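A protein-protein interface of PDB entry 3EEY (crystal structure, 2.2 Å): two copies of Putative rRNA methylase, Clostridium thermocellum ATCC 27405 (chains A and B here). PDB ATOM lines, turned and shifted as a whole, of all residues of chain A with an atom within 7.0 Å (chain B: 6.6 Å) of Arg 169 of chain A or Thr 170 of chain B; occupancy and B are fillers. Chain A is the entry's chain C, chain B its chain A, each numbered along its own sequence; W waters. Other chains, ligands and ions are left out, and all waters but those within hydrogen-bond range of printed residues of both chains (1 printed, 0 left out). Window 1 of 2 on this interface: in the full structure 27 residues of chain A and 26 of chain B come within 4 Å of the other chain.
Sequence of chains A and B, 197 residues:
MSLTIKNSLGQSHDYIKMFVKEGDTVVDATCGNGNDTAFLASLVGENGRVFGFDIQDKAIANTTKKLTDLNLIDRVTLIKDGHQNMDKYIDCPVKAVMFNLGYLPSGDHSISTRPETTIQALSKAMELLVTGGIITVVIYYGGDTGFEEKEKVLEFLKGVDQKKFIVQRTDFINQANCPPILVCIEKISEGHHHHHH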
ATOM      1  N   GLN A  11      -2.355   2.175   4.138  1.00  0.00           N
ATOM      2  CA  GLN A  11      -3.232   2.840   5.088  1.00  0.00           C
ATOM      3  C   GLN A  11      -2.520   3.877   5.950  1.00  0.00           C
ATOM      4  O   GLN A  11      -3.116   4.893   6.298  1.00  0.00           O
ATOM      5  CB  GLN A  11      -3.930   1.810   5.970  1.00  0.00           C
ATOM      6  CG  GLN A  11      -5.045   1.054   5.271  1.00  0.00           C
ATOM      7  CD  GLN A  11      -5.897   0.263   6.232  1.00  0.00           C
ATOM      8  OE1 GLN A  11      -6.440   0.814   7.187  1.00  0.00           O
ATOM      9  NE2 GLN A  11      -6.022  -1.036   5.984  1.00  0.00           N
ATOM     10  N   TYR A  15      -3.828   7.674   6.603  1.00  0.00           N
ATOM     11  CA  TYR A  15      -3.978   8.263   7.942  1.00  0.00           C
ATOM     12  C   TYR A  15      -3.132   9.518   8.123  1.00  0.00           C
ATOM     13  O   TYR A  15      -3.552  10.458   8.788  1.00  0.00           O
ATOM     14  CB  TYR A  15      -3.610   7.256   9.036  1.00  0.00           C
ATOM     15  CG  TYR A  15      -4.735   6.346   9.480  1.00  0.00           C
ATOM     16  CD1 TYR A  15      -4.792   5.024   9.053  1.00  0.00           C
ATOM     17  CD2 TYR A  15      -5.727   6.801  10.351  1.00  0.00           C
ATOM     18  CE1 TYR A  15      -5.806   4.182   9.461  1.00  0.00           C
ATOM     19  CE2 TYR A  15      -6.753   5.961  10.769  1.00  0.00           C
ATOM     20  CZ  TYR A  15      -6.784   4.650  10.321  1.00  0.00           C
ATOM     21  OH  TYR A  15      -7.786   3.797  10.734  1.00  0.00           O
ATOM     22  N   LYS A 150       7.584  -7.065  17.368  1.00  0.00           N
ATOM     23  CA  LYS A 150       6.116  -7.033  17.404  1.00  0.00           C
ATOM     24  C   LYS A 150       5.552  -7.299  18.796  1.00  0.00           C
ATOM     25  O   LYS A 150       4.760  -6.511  19.302  1.00  0.00           O
ATOM     26  CB  LYS A 150       5.515  -8.037  16.410  1.00  0.00           C
ATOM     27  CG  LYS A 150       3.982  -7.960  16.312  1.00  0.00           C
ATOM     28  CD  LYS A 150       3.351  -9.137  15.586  1.00  0.00           C
ATOM     29  CE  LYS A 150       3.094 -10.317  16.516  1.00  0.00           C
ATOM     30  NZ  LYS A 150       1.672 -10.389  16.953  1.00  0.00           N
ATOM     31  N   LEU A 154       3.850  -4.124  20.948  1.00  0.00           N
ATOM     32  CA  LEU A 154       2.436  -4.289  21.238  1.00  0.00           C
ATOM     33  C   LEU A 154       2.164  -4.407  22.732  1.00  0.00           C
ATOM     34  O   LEU A 154       1.227  -3.775  23.220  1.00  0.00           O
ATOM     35  CB  LEU A 154       1.835  -5.468  20.463  1.00  0.00           C
ATOM     36  CG  LEU A 154       1.635  -5.260  18.950  1.00  0.00           C
ATOM     37  CD1 LEU A 154       1.091  -6.513  18.317  1.00  0.00           C
ATOM     38  CD2 LEU A 154       0.710  -4.090  18.643  1.00  0.00           C
ATOM     39  N   LYS A 158      -0.110  -1.566  24.683  1.00  0.00           N
ATOM     40  CA  LYS A 158      -1.315  -1.937  25.425  1.00  0.00           C
ATOM     41  C   LYS A 158      -1.400  -1.218  26.772  1.00  0.00           C
ATOM     42  O   LYS A 158      -2.495  -1.066  27.323  1.00  0.00           O
ATOM     43  CB  LYS A 158      -1.409  -3.455  25.607  1.00  0.00           C
ATOM     44  CG  LYS A 158      -1.905  -4.186  24.367  1.00  0.00           C
ATOM     45  CD  LYS A 158      -1.886  -5.694  24.549  1.00  0.00           C
ATOM     46  CE  LYS A 158      -2.248  -6.420  23.252  1.00  0.00           C
ATOM     47  NZ  LYS A 158      -3.681  -6.242  22.875  1.00  0.00           N
ATOM     48  N   VAL A 167      -4.910   4.120  20.990  1.00  0.00           N
ATOM     49  CA  VAL A 167      -4.040   3.183  20.269  1.00  0.00           C
ATOM     50  C   VAL A 167      -4.902   2.183  19.494  1.00  0.00           C
ATOM     51  O   VAL A 167      -5.606   1.369  20.078  1.00  0.00           O
ATOM     52  CB  VAL A 167      -3.039   2.492  21.204  1.00  0.00           C
ATOM     53  CG1 VAL A 167      -2.103   1.579  20.422  1.00  0.00           C
ATOM     54  CG2 VAL A 167      -2.226   3.548  21.960  1.00  0.00           C
ATOM     55  N   GLN A 168      -4.854   2.286  18.167  1.00  0.00           N
ATOM     56  CA  GLN A 168      -5.677   1.474  17.276  1.00  0.00           C
ATOM     57  C   GLN A 168      -4.827   0.487  16.495  1.00  0.00           C
ATOM     58  O   GLN A 168      -3.879   0.873  15.827  1.00  0.00           O
ATOM     59  CB  GLN A 168      -6.418   2.383  16.288  1.00  0.00           C
ATOM     60  CG  GLN A 168      -7.479   1.690  15.466  1.00  0.00           C
ATOM     61  CD  GLN A 168      -7.807   2.426  14.193  1.00  0.00           C
ATOM     62  OE1 GLN A 168      -8.839   3.075  14.095  1.00  0.00           O
ATOM     63  NE2 GLN A 168      -6.929   2.337  13.212  1.00  0.00           N
ATOM     64  N   ARG A 169      -5.190  -0.786  16.546  1.00  0.00           N
ATOM     65  CA  ARG A 169      -4.499  -1.805  15.766  1.00  0.00           C
ATOM     66  C   ARG A 169      -5.345  -2.282  14.598  1.00  0.00           C
ATOM     67  O   ARG A 169      -6.511  -2.590  14.769  1.00  0.00           O
ATOM     68  CB  ARG A 169      -4.164  -3.018  16.643  1.00  0.00           C
ATOM     69  CG  ARG A 169      -3.555  -4.173  15.835  1.00  0.00           C
ATOM     70  CD  ARG A 169      -3.090  -5.317  16.708  1.00  0.00           C
ATOM     71  NE  ARG A 169      -4.226  -5.955  17.363  1.00  0.00           N
ATOM     72  CZ  ARG A 169      -4.142  -6.933  18.257  1.00  0.00           C
ATOM     73  NH1 ARG A 169      -2.958  -7.428  18.614  1.00  0.00           N
ATOM     74  NH2 ARG A 169      -5.258  -7.423  18.787  1.00  0.00           N
ATOM     75  N   THR A 170      -4.738  -2.391  13.421  1.00  0.00           N
ATOM     76  CA  THR A 170      -5.420  -2.863  12.227  1.00  0.00           C
ATOM     77  C   THR A 170      -4.683  -4.098  11.714  1.00  0.00           C
ATOM     78  O   THR A 170      -3.480  -4.065  11.548  1.00  0.00           O
ATOM     79  CB  THR A 170      -5.452  -1.768  11.142  1.00  0.00           C
ATOM     80  OG1 THR A 170      -6.157  -0.620  11.642  1.00  0.00           O
ATOM     81  CG2 THR A 170      -6.134  -2.262   9.894  1.00  0.00           C
ATOM     82  N   ASP A 171      -5.425  -5.165  11.440  1.00  0.00           N
ATOM     83  CA  ASP A 171      -4.863  -6.488  11.265  1.00  0.00           C
ATOM     84  C   ASP A 171      -5.686  -7.222  10.221  1.00  0.00           C
ATOM     85  O   ASP A 171      -6.900  -7.178  10.251  1.00  0.00           O
ATOM     86  CB  ASP A 171      -4.910  -7.238  12.609  1.00  0.00           C
ATOM     87  CG  ASP A 171      -3.879  -8.348  12.714  1.00  0.00           C
ATOM     88  OD1 ASP A 171      -3.207  -8.676  11.710  1.00  0.00           O
ATOM     89  OD2 ASP A 171      -3.742  -8.897  13.826  1.00  0.00           O
ATOM     90  N   ILE A 181       1.210  -5.265  10.199  1.00  0.00           N
ATOM     91  CA  ILE A 181       0.205  -4.732  11.113  1.00  0.00           C
ATOM     92  C   ILE A 181       0.343  -3.208  11.169  1.00  0.00           C
ATOM     93  O   ILE A 181       1.453  -2.686  11.142  1.00  0.00           O
ATOM     94  CB  ILE A 181       0.384  -5.359  12.534  1.00  0.00           C
ATOM     95  CG1 ILE A 181      -0.084  -6.809  12.545  1.00  0.00           C
ATOM     96  CG2 ILE A 181      -0.395  -4.604  13.629  1.00  0.00           C
ATOM     97  CD1 ILE A 181       0.339  -7.571  13.794  1.00  0.00           C
ATOM     98  N   LEU A 182      -0.782  -2.496  11.214  1.00  0.00           N
ATOM     99  CA  LEU A 182      -0.763  -1.051  11.411  1.00  0.00           C
ATOM    100  C   LEU A 182      -1.205  -0.697  12.816  1.00  0.00           C
ATOM    101  O   LEU A 182      -2.235  -1.173  13.282  1.00  0.00           O
ATOM    102  CB  LEU A 182      -1.664  -0.350  10.399  1.00  0.00           C
ATOM    103  CG  LEU A 182      -1.829   1.175  10.511  1.00  0.00           C
ATOM    104  CD1 LEU A 182      -0.519   1.931  10.268  1.00  0.00           C
ATOM    105  CD2 LEU A 182      -2.885   1.637   9.546  1.00  0.00           C
ATOM    106  N   VAL A 183      -0.416   0.135  13.490  1.00  0.00           N
ATOM    107  CA  VAL A 183      -0.829   0.737  14.757  1.00  0.00           C
ATOM    108  C   VAL A 183      -0.895   2.266  14.598  1.00  0.00           C
ATOM    109  O   VAL A 183       0.063   2.888  14.147  1.00  0.00           O
ATOM    110  CB  VAL A 183       0.105   0.345  15.927  1.00  0.00           C
ATOM    111  CG1 VAL A 183      -0.348   0.999  17.217  1.00  0.00           C
ATOM    112  CG2 VAL A 183       0.137  -1.174  16.129  1.00  0.00           C
ATOM    113  N   CYS A 184      -2.039   2.853  14.946  1.00  0.00           N
ATOM    114  CA  CYS A 184      -2.216   4.304  14.924  1.00  0.00           C
ATOM    115  C   CYS A 184      -2.362   4.828  16.338  1.00  0.00           C
ATOM    116  O   CYS A 184      -3.209   4.358  17.090  1.00  0.00           O
ATOM    117  CB  CYS A 184      -3.436   4.705  14.097  1.00  0.00           C
ATOM    118  SG  CYS A 184      -3.244   4.341  12.365  1.00  0.00           S
ATOM    119  N   LYS B   6     -12.214   7.411  15.025  1.00  0.00           N
ATOM    120  CA  LYS B   6     -13.513   6.995  15.550  1.00  0.00           C
ATOM    121  C   LYS B   6     -13.453   5.606  16.145  1.00  0.00           C
ATOM    122  O   LYS B   6     -12.577   4.809  15.804  1.00  0.00           O
ATOM    123  CB  LYS B   6     -14.580   7.030  14.455  1.00  0.00           C
ATOM    124  CG  LYS B   6     -14.886   8.410  13.936  1.00  0.00           C
ATOM    125  CD  LYS B   6     -15.936   8.388  12.847  1.00  0.00           C
ATOM    126  CE  LYS B   6     -15.968   9.737  12.131  1.00  0.00           C
ATOM    127  NZ  LYS B   6     -16.838   9.745  10.926  1.00  0.00           N
ATOM    128  N   SER B   8     -15.185   1.723  16.757  1.00  0.00           N
ATOM    129  CA  SER B   8     -15.630   0.703  15.805  1.00  0.00           C
ATOM    130  C   SER B   8     -16.997   1.005  15.200  1.00  0.00           C
ATOM    131  O   SER B   8     -17.160   0.963  13.979  1.00  0.00           O
ATOM    132  CB  SER B   8     -15.619  -0.669  16.461  1.00  0.00           C
ATOM    133  OG  SER B   8     -14.293  -1.041  16.782  1.00  0.00           O
ATOM    134  N   GLN B  11     -16.648   3.896  12.795  1.00  0.00           N
ATOM    135  CA  GLN B  11     -15.866   3.442  11.648  1.00  0.00           C
ATOM    136  C   GLN B  11     -16.638   2.536  10.683  1.00  0.00           C
ATOM    137  O   GLN B  11     -16.423   2.612   9.467  1.00  0.00           O
ATOM    138  CB  GLN B  11     -14.592   2.748  12.117  1.00  0.00           C
ATOM    139  CG  GLN B  11     -13.513   3.696  12.592  1.00  0.00           C
ATOM    140  CD  GLN B  11     -12.175   3.031  12.699  1.00  0.00           C
ATOM    141  OE1 GLN B  11     -11.676   2.437  11.736  1.00  0.00           O
ATOM    142  NE2 GLN B  11     -11.573   3.126  13.873  1.00  0.00           N
ATOM    143  N   TYR B  15     -16.923   3.134   6.648  1.00  0.00           N
ATOM    144  CA  TYR B  15     -16.667   2.079   5.668  1.00  0.00           C
ATOM    145  C   TYR B  15     -17.858   1.820   4.754  1.00  0.00           C
ATOM    146  O   TYR B  15     -17.676   1.540   3.573  1.00  0.00           O
ATOM    147  CB  TYR B  15     -16.249   0.779   6.358  1.00  0.00           C
ATOM    148  CG  TYR B  15     -14.770   0.694   6.651  1.00  0.00           C
ATOM    149  CD1 TYR B  15     -14.276   0.929   7.935  1.00  0.00           C
ATOM    150  CD2 TYR B  15     -13.858   0.375   5.643  1.00  0.00           C
ATOM    151  CE1 TYR B  15     -12.911   0.859   8.211  1.00  0.00           C
ATOM    152  CE2 TYR B  15     -12.489   0.292   5.911  1.00  0.00           C
ATOM    153  CZ  TYR B  15     -12.022   0.535   7.194  1.00  0.00           C
ATOM    154  OH  TYR B  15     -10.672   0.465   7.470  1.00  0.00           O
ATOM    155  N   GLN B 168     -10.435  -7.584   7.613  1.00  0.00           N
ATOM    156  CA  GLN B 168      -9.653  -6.638   8.367  1.00  0.00           C
ATOM    157  C   GLN B 168     -10.261  -6.417   9.740  1.00  0.00           C
ATOM    158  O   GLN B 168     -11.425  -6.053   9.854  1.00  0.00           O
ATOM    159  CB  GLN B 168      -9.571  -5.326   7.611  1.00  0.00           C
ATOM    160  CG  GLN B 168      -8.743  -4.267   8.274  1.00  0.00           C
ATOM    161  CD  GLN B 168      -9.124  -2.882   7.799  1.00  0.00           C
ATOM    162  OE1 GLN B 168      -8.462  -2.304   6.946  1.00  0.00           O
ATOM    163  NE2 GLN B 168     -10.213  -2.351   8.337  1.00  0.00           N
ATOM    164  N   ARG B 169      -9.464  -6.645  10.778  1.00  0.00           N
ATOM    165  CA  ARG B 169      -9.876  -6.365  12.138  1.00  0.00           C
ATOM    166  C   ARG B 169      -9.287  -5.041  12.644  1.00  0.00           C
ATOM    167  O   ARG B 169      -8.113  -4.765  12.450  1.00  0.00           O
ATOM    168  CB  ARG B 169      -9.474  -7.503  13.059  1.00  0.00           C
ATOM    169  CG  ARG B 169     -10.053  -7.355  14.462  1.00  0.00           C
ATOM    170  CD  ARG B 169      -9.368  -8.256  15.463  1.00  0.00           C
ATOM    171  NE  ARG B 169      -7.906  -8.238  15.366  1.00  0.00           N
ATOM    172  CZ  ARG B 169      -7.118  -9.190  15.867  1.00  0.00           C
ATOM    173  NH1 ARG B 169      -7.649 -10.227  16.505  1.00  0.00           N
ATOM    174  NH2 ARG B 169      -5.804  -9.112  15.735  1.00  0.00           N
ATOM    175  N   THR B 170     -10.125  -4.230  13.281  1.00  0.00           N
ATOM    176  CA  THR B 170      -9.711  -2.981  13.882  1.00  0.00           C
ATOM    177  C   THR B 170      -9.998  -3.076  15.383  1.00  0.00           C
ATOM    178  O   THR B 170     -11.072  -3.505  15.786  1.00  0.00           O
ATOM    179  CB  THR B 170     -10.434  -1.777  13.220  1.00  0.00           C
ATOM    180  OG1 THR B 170     -10.123  -1.752  11.821  1.00  0.00           O
ATOM    181  CG2 THR B 170      -9.994  -0.462  13.833  1.00  0.00           C
ATOM    182  N   ASP B 171      -9.024  -2.677  16.194  1.00  0.00           N
ATOM    183  CA  ASP B 171      -8.992  -3.004  17.602  1.00  0.00           C
ATOM    184  C   ASP B 171      -8.305  -1.875  18.365  1.00  0.00           C
ATOM    185  O   ASP B 171      -7.258  -1.396  17.950  1.00  0.00           O
ATOM    186  CB  ASP B 171      -8.203  -4.307  17.779  1.00  0.00           C
ATOM    187  CG  ASP B 171      -8.528  -5.030  19.069  1.00  0.00           C
ATOM    188  OD1 ASP B 171      -9.367  -4.535  19.859  1.00  0.00           O
ATOM    189  OD2 ASP B 171      -7.935  -6.108  19.286  1.00  0.00           O
ATOM    190  N   PHE B 172      -8.905  -1.458  19.478  1.00  0.00           N
ATOM    191  CA  PHE B 172      -8.319  -0.451  20.355  1.00  0.00           C
ATOM    192  C   PHE B 172      -7.677  -1.128  21.544  1.00  0.00           C
ATOM    193  O   PHE B 172      -8.353  -1.551  22.471  1.00  0.00           O
ATOM    194  CB  PHE B 172      -9.362   0.587  20.759  1.00  0.00           C
ATOM    195  CG  PHE B 172      -9.962   1.295  19.575  1.00  0.00           C
ATOM    196  CD1 PHE B 172      -9.310   2.382  18.991  1.00  0.00           C
ATOM    197  CD2 PHE B 172     -11.151   0.838  19.006  1.00  0.00           C
ATOM    198  CE1 PHE B 172      -9.851   3.031  17.864  1.00  0.00           C
ATOM    199  CE2 PHE B 172     -11.692   1.469  17.872  1.00  0.00           C
ATOM    200  CZ  PHE B 172     -11.043   2.559  17.311  1.00  0.00           C
ATOM    201  N   ILE B 173      -6.353  -1.230  21.489  1.00  0.00           N
ATOM    202  CA  ILE B 173      -5.617  -2.179  22.317  1.00  0.00           C
ATOM    203  C   ILE B 173      -5.197  -1.620  23.676  1.00  0.00           C
ATOM    204  O   ILE B 173      -4.789  -2.381  24.545  1.00  0.00           O
ATOM    205  CB  ILE B 173      -4.397  -2.789  21.551  1.00  0.00           C
ATOM    206  CG1 ILE B 173      -3.380  -1.706  21.179  1.00  0.00           C
ATOM    207  CG2 ILE B 173      -4.866  -3.519  20.304  1.00  0.00           C
ATOM    208  CD1 ILE B 173      -2.093  -2.218  20.537  1.00  0.00           C
ATOM    209  N   PRO B 180     -15.484  -2.323  21.748  1.00  0.00           N
ATOM    210  CA  PRO B 180     -16.014  -3.039  20.581  1.00  0.00           C
ATOM    211  C   PRO B 180     -15.022  -3.155  19.421  1.00  0.00           C
ATOM    212  O   PRO B 180     -14.249  -2.233  19.150  1.00  0.00           O
ATOM    213  CB  PRO B 180     -17.239  -2.203  20.180  1.00  0.00           C
ATOM    214  CG  PRO B 180     -17.642  -1.514  21.437  1.00  0.00           C
ATOM    215  CD  PRO B 180     -16.367  -1.214  22.161  1.00  0.00           C
ATOM    216  N   ILE B 181     -15.047  -4.310  18.769  1.00  0.00           N
ATOM    217  CA  ILE B 181     -14.128  -4.650  17.686  1.00  0.00           C
ATOM    218  C   ILE B 181     -14.819  -4.509  16.333  1.00  0.00           C
ATOM    219  O   ILE B 181     -15.946  -4.940  16.191  1.00  0.00           O
ATOM    220  CB  ILE B 181     -13.621  -6.087  17.891  1.00  0.00           C
ATOM    221  CG1 ILE B 181     -12.630  -6.125  19.059  1.00  0.00           C
ATOM    222  CG2 ILE B 181     -12.985  -6.658  16.631  1.00  0.00           C
ATOM    223  CD1 ILE B 181     -12.320  -7.524  19.543  1.00  0.00           C
ATOM    224  N   LEU B 182     -14.143  -3.906  15.349  1.00  0.00           N
ATOM    225  CA  LEU B 182     -14.660  -3.834  13.979  1.00  0.00           C
ATOM    226  C   LEU B 182     -13.990  -4.827  13.025  1.00  0.00           C
ATOM    227  O   LEU B 182     -12.780  -4.808  12.863  1.00  0.00           O
ATOM    228  CB  LEU B 182     -14.504  -2.426  13.409  1.00  0.00           C
ATOM    229  CG  LEU B 182     -14.952  -2.234  11.954  1.00  0.00           C
ATOM    230  CD1 LEU B 182     -16.459  -2.441  11.769  1.00  0.00           C
ATOM    231  CD2 LEU B 182     -14.536  -0.878  11.445  1.00  0.00           C
ATOM    232  N   VAL B 183     -14.791  -5.672  12.383  1.00  0.00           N
ATOM    233  CA  VAL B 183     -14.300  -6.519  11.305  1.00  0.00           C
ATOM    234  C   VAL B 183     -14.908  -6.040   9.982  1.00  0.00           C
ATOM    235  O   VAL B 183     -16.107  -5.816   9.890  1.00  0.00           O
ATOM    236  CB  VAL B 183     -14.573  -8.024  11.559  1.00  0.00           C
ATOM    237  CG1 VAL B 183     -13.990  -8.866  10.462  1.00  0.00           C
ATOM    238  CG2 VAL B 183     -13.957  -8.470  12.880  1.00  0.00           C
ATOM    239  N   CYS B 184     -14.059  -5.834   8.983  1.00  0.00           N
ATOM    240  CA  CYS B 184     -14.494  -5.466   7.647  1.00  0.00           C
ATOM    241  C   CYS B 184     -14.168  -6.591   6.690  1.00  0.00           C
ATOM    242  O   CYS B 184     -13.016  -6.989   6.578  1.00  0.00           O
ATOM    243  CB  CYS B 184     -13.797  -4.192   7.184  1.00  0.00           C
ATOM    244  SG  CYS B 184     -14.337  -2.727   8.031  1.00  0.00           S
HETATM  245  O   HOH W   1      -9.904   5.301  11.653  1.00  0.00           O
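Thr 170 of chain B touches just these residues of chain A: Gln 168 and Arg 169. Of the printed residues of chain A, Asp 171 of chain B touches Val 167 (3.9 Å), Gln 168 (3.3 Å) and Arg 169 (2.6 Å). Of the printed residues of chain B, Gln 168 of chain A touches Gln 11, Thr 170, Asp 171 and Phe 172. Printed residues of chain A within 4 Å of Gln 11 of chain B: Gln 168 (2.7 Å). Of the printed residues of chain A, Ile 173 of chain B touches Leu 154, Lys 158, Val 167 and Arg 169. Pro 180 of chain B touches none of the printed residues of chain A. Leu 182 of chain A touches none of the printed residues of chain B. The nearest residue of chain B that does not touch Arg 169 of chain A is Phe 172 of chain B (4.8 Å). The nearest printed residue of chain B that does not touch Thr 170 of chain A is Thr 170 of chain B (4.1 Å).
The backbone carbonyl oxygen (O) of Lys 6 of chain B lies within hydrogen-bond range of the side-chain amide nitrogen (NE2) of Gln 11 of chain B. OH of Tyr 15 of chain B lies within hydrogen-bond range of NE2 of Gln 168 of chain B (3.0 Å). The backbone carbonyl oxygen (O) of Gln 168 of chain B lies within hydrogen-bond range of the backbone NH (N) of Cys 184 of chain B, 2.8 Å away. N of Thr 170 of chain B lies within hydrogen-bond range of O of Leu 182 of chain B. The side-chain hydroxyl of Tyr 15 of chain A is in hydrogen-bond range of the side-chain amide nitrogen of Gln 168 of chain A (3.0 Å). NE2 of Gln 168 of chain A sits at hydrogen-bond distance from OG1 of Thr 170 of chain A, 3.4 Å away.
Among the printed residues, pairs that only touch across the chains: Val 167 of chain A with Phe 172 of chain B, Thr 170 of chain A with Arg 169 of chain B, Arg 169 of chain A with Thr 170 of chain B, Gln 168 of chain A with Asp 171 of chain B, Asp 171 of chain A with Gln 168 of chain B, Lys 158 of chain A with Ile 173 of chain B, Arg 169 of chain A with Arg 169 of chain B, Gln 168 of chain A with Phe 172 of chain B, Gln 168 of chain A with Thr 170 of chain B, Thr 170 of chain A with Gln 168 of chain B, Arg 169 of chain A with Ile 173 of chain B, Val 167 of chain A with Asp 171 of chain B and Leu 154 of chain A with Ile 173 of chain B.
OE1 of Gln 168 of chain A lies within hydrogen-bond range of NE2 of Gln 11 of chain B (2.7 Å). OE1 of Gln 168 of chain B sits at hydrogen-bond distance from NE2 of Gln 11 of chain A (2.9 Å). OD2 of Asp 171 of chain A lies within salt-bridge range of NH2 of Arg 169 of chain B (2.8 Å). NH2 of Arg 169 of chain A is in salt-bridge range of OD2 of Asp 171 of chain B (3.0 Å). The backbone NH of Ile 173 of chain B sits at hydrogen-bond distance from the backbone carbonyl oxygen of Val 167 of chain A, 3.1 Å away.
Water W1 lies within hydrogen-bond range of OH of Tyr 15 of chain A (2.8 Å), OE1 of Gln 11 of chain B (3.4 Å) and OE1 of Gln 168 of chain A (3.5 Å).
Gln 168 of chain A touches Thr 170 of chain B, and with the chains exchanged Thr 170 of chain A touches Gln 168 of chain B. Gln 168 of chain A touches Asp 171 of chain B, and with the chains exchanged Asp 171 of chain A touches Gln 168 of chain B. Arg 169 of chain B touches its own counterpart, Arg 169 of chain A. Arg 169 of chain A touches Thr 170 of chain B, and with the chains exchanged Thr 170 of chain A touches Arg 169 of chain B. 10 positions are printed for both chains. Of the 18 pairs that touch across the chains among the printed residues, 11 have their exchanged pair printed and touching as well.
Of the 15 printed residues of chain B, 7 touch a printed residue of chain A. Printed residues of chain B that touch a printed residue of chain A: Gln 11, Gln 168, Arg 169, Thr 170, Asp 171, Phe 172 and Ile 173. Hydrophobic or aromatic side chains of chain A within 4 Å of the printed part of chain B: Leu 154 and Val 167. Along chain A the printed residues that touch a printed residue of chain B span positions 11 to 171. Among the printed residues, 18 pairs touch across the chains. Among the printed residues, Asp or Glu carboxylates within 4 Å of a Lys or Arg side-chain nitrogen of the other chain: Arg 169 of chain A with Asp 171 of chain B and Asp 171 of chain A with Arg 169 of chain B.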
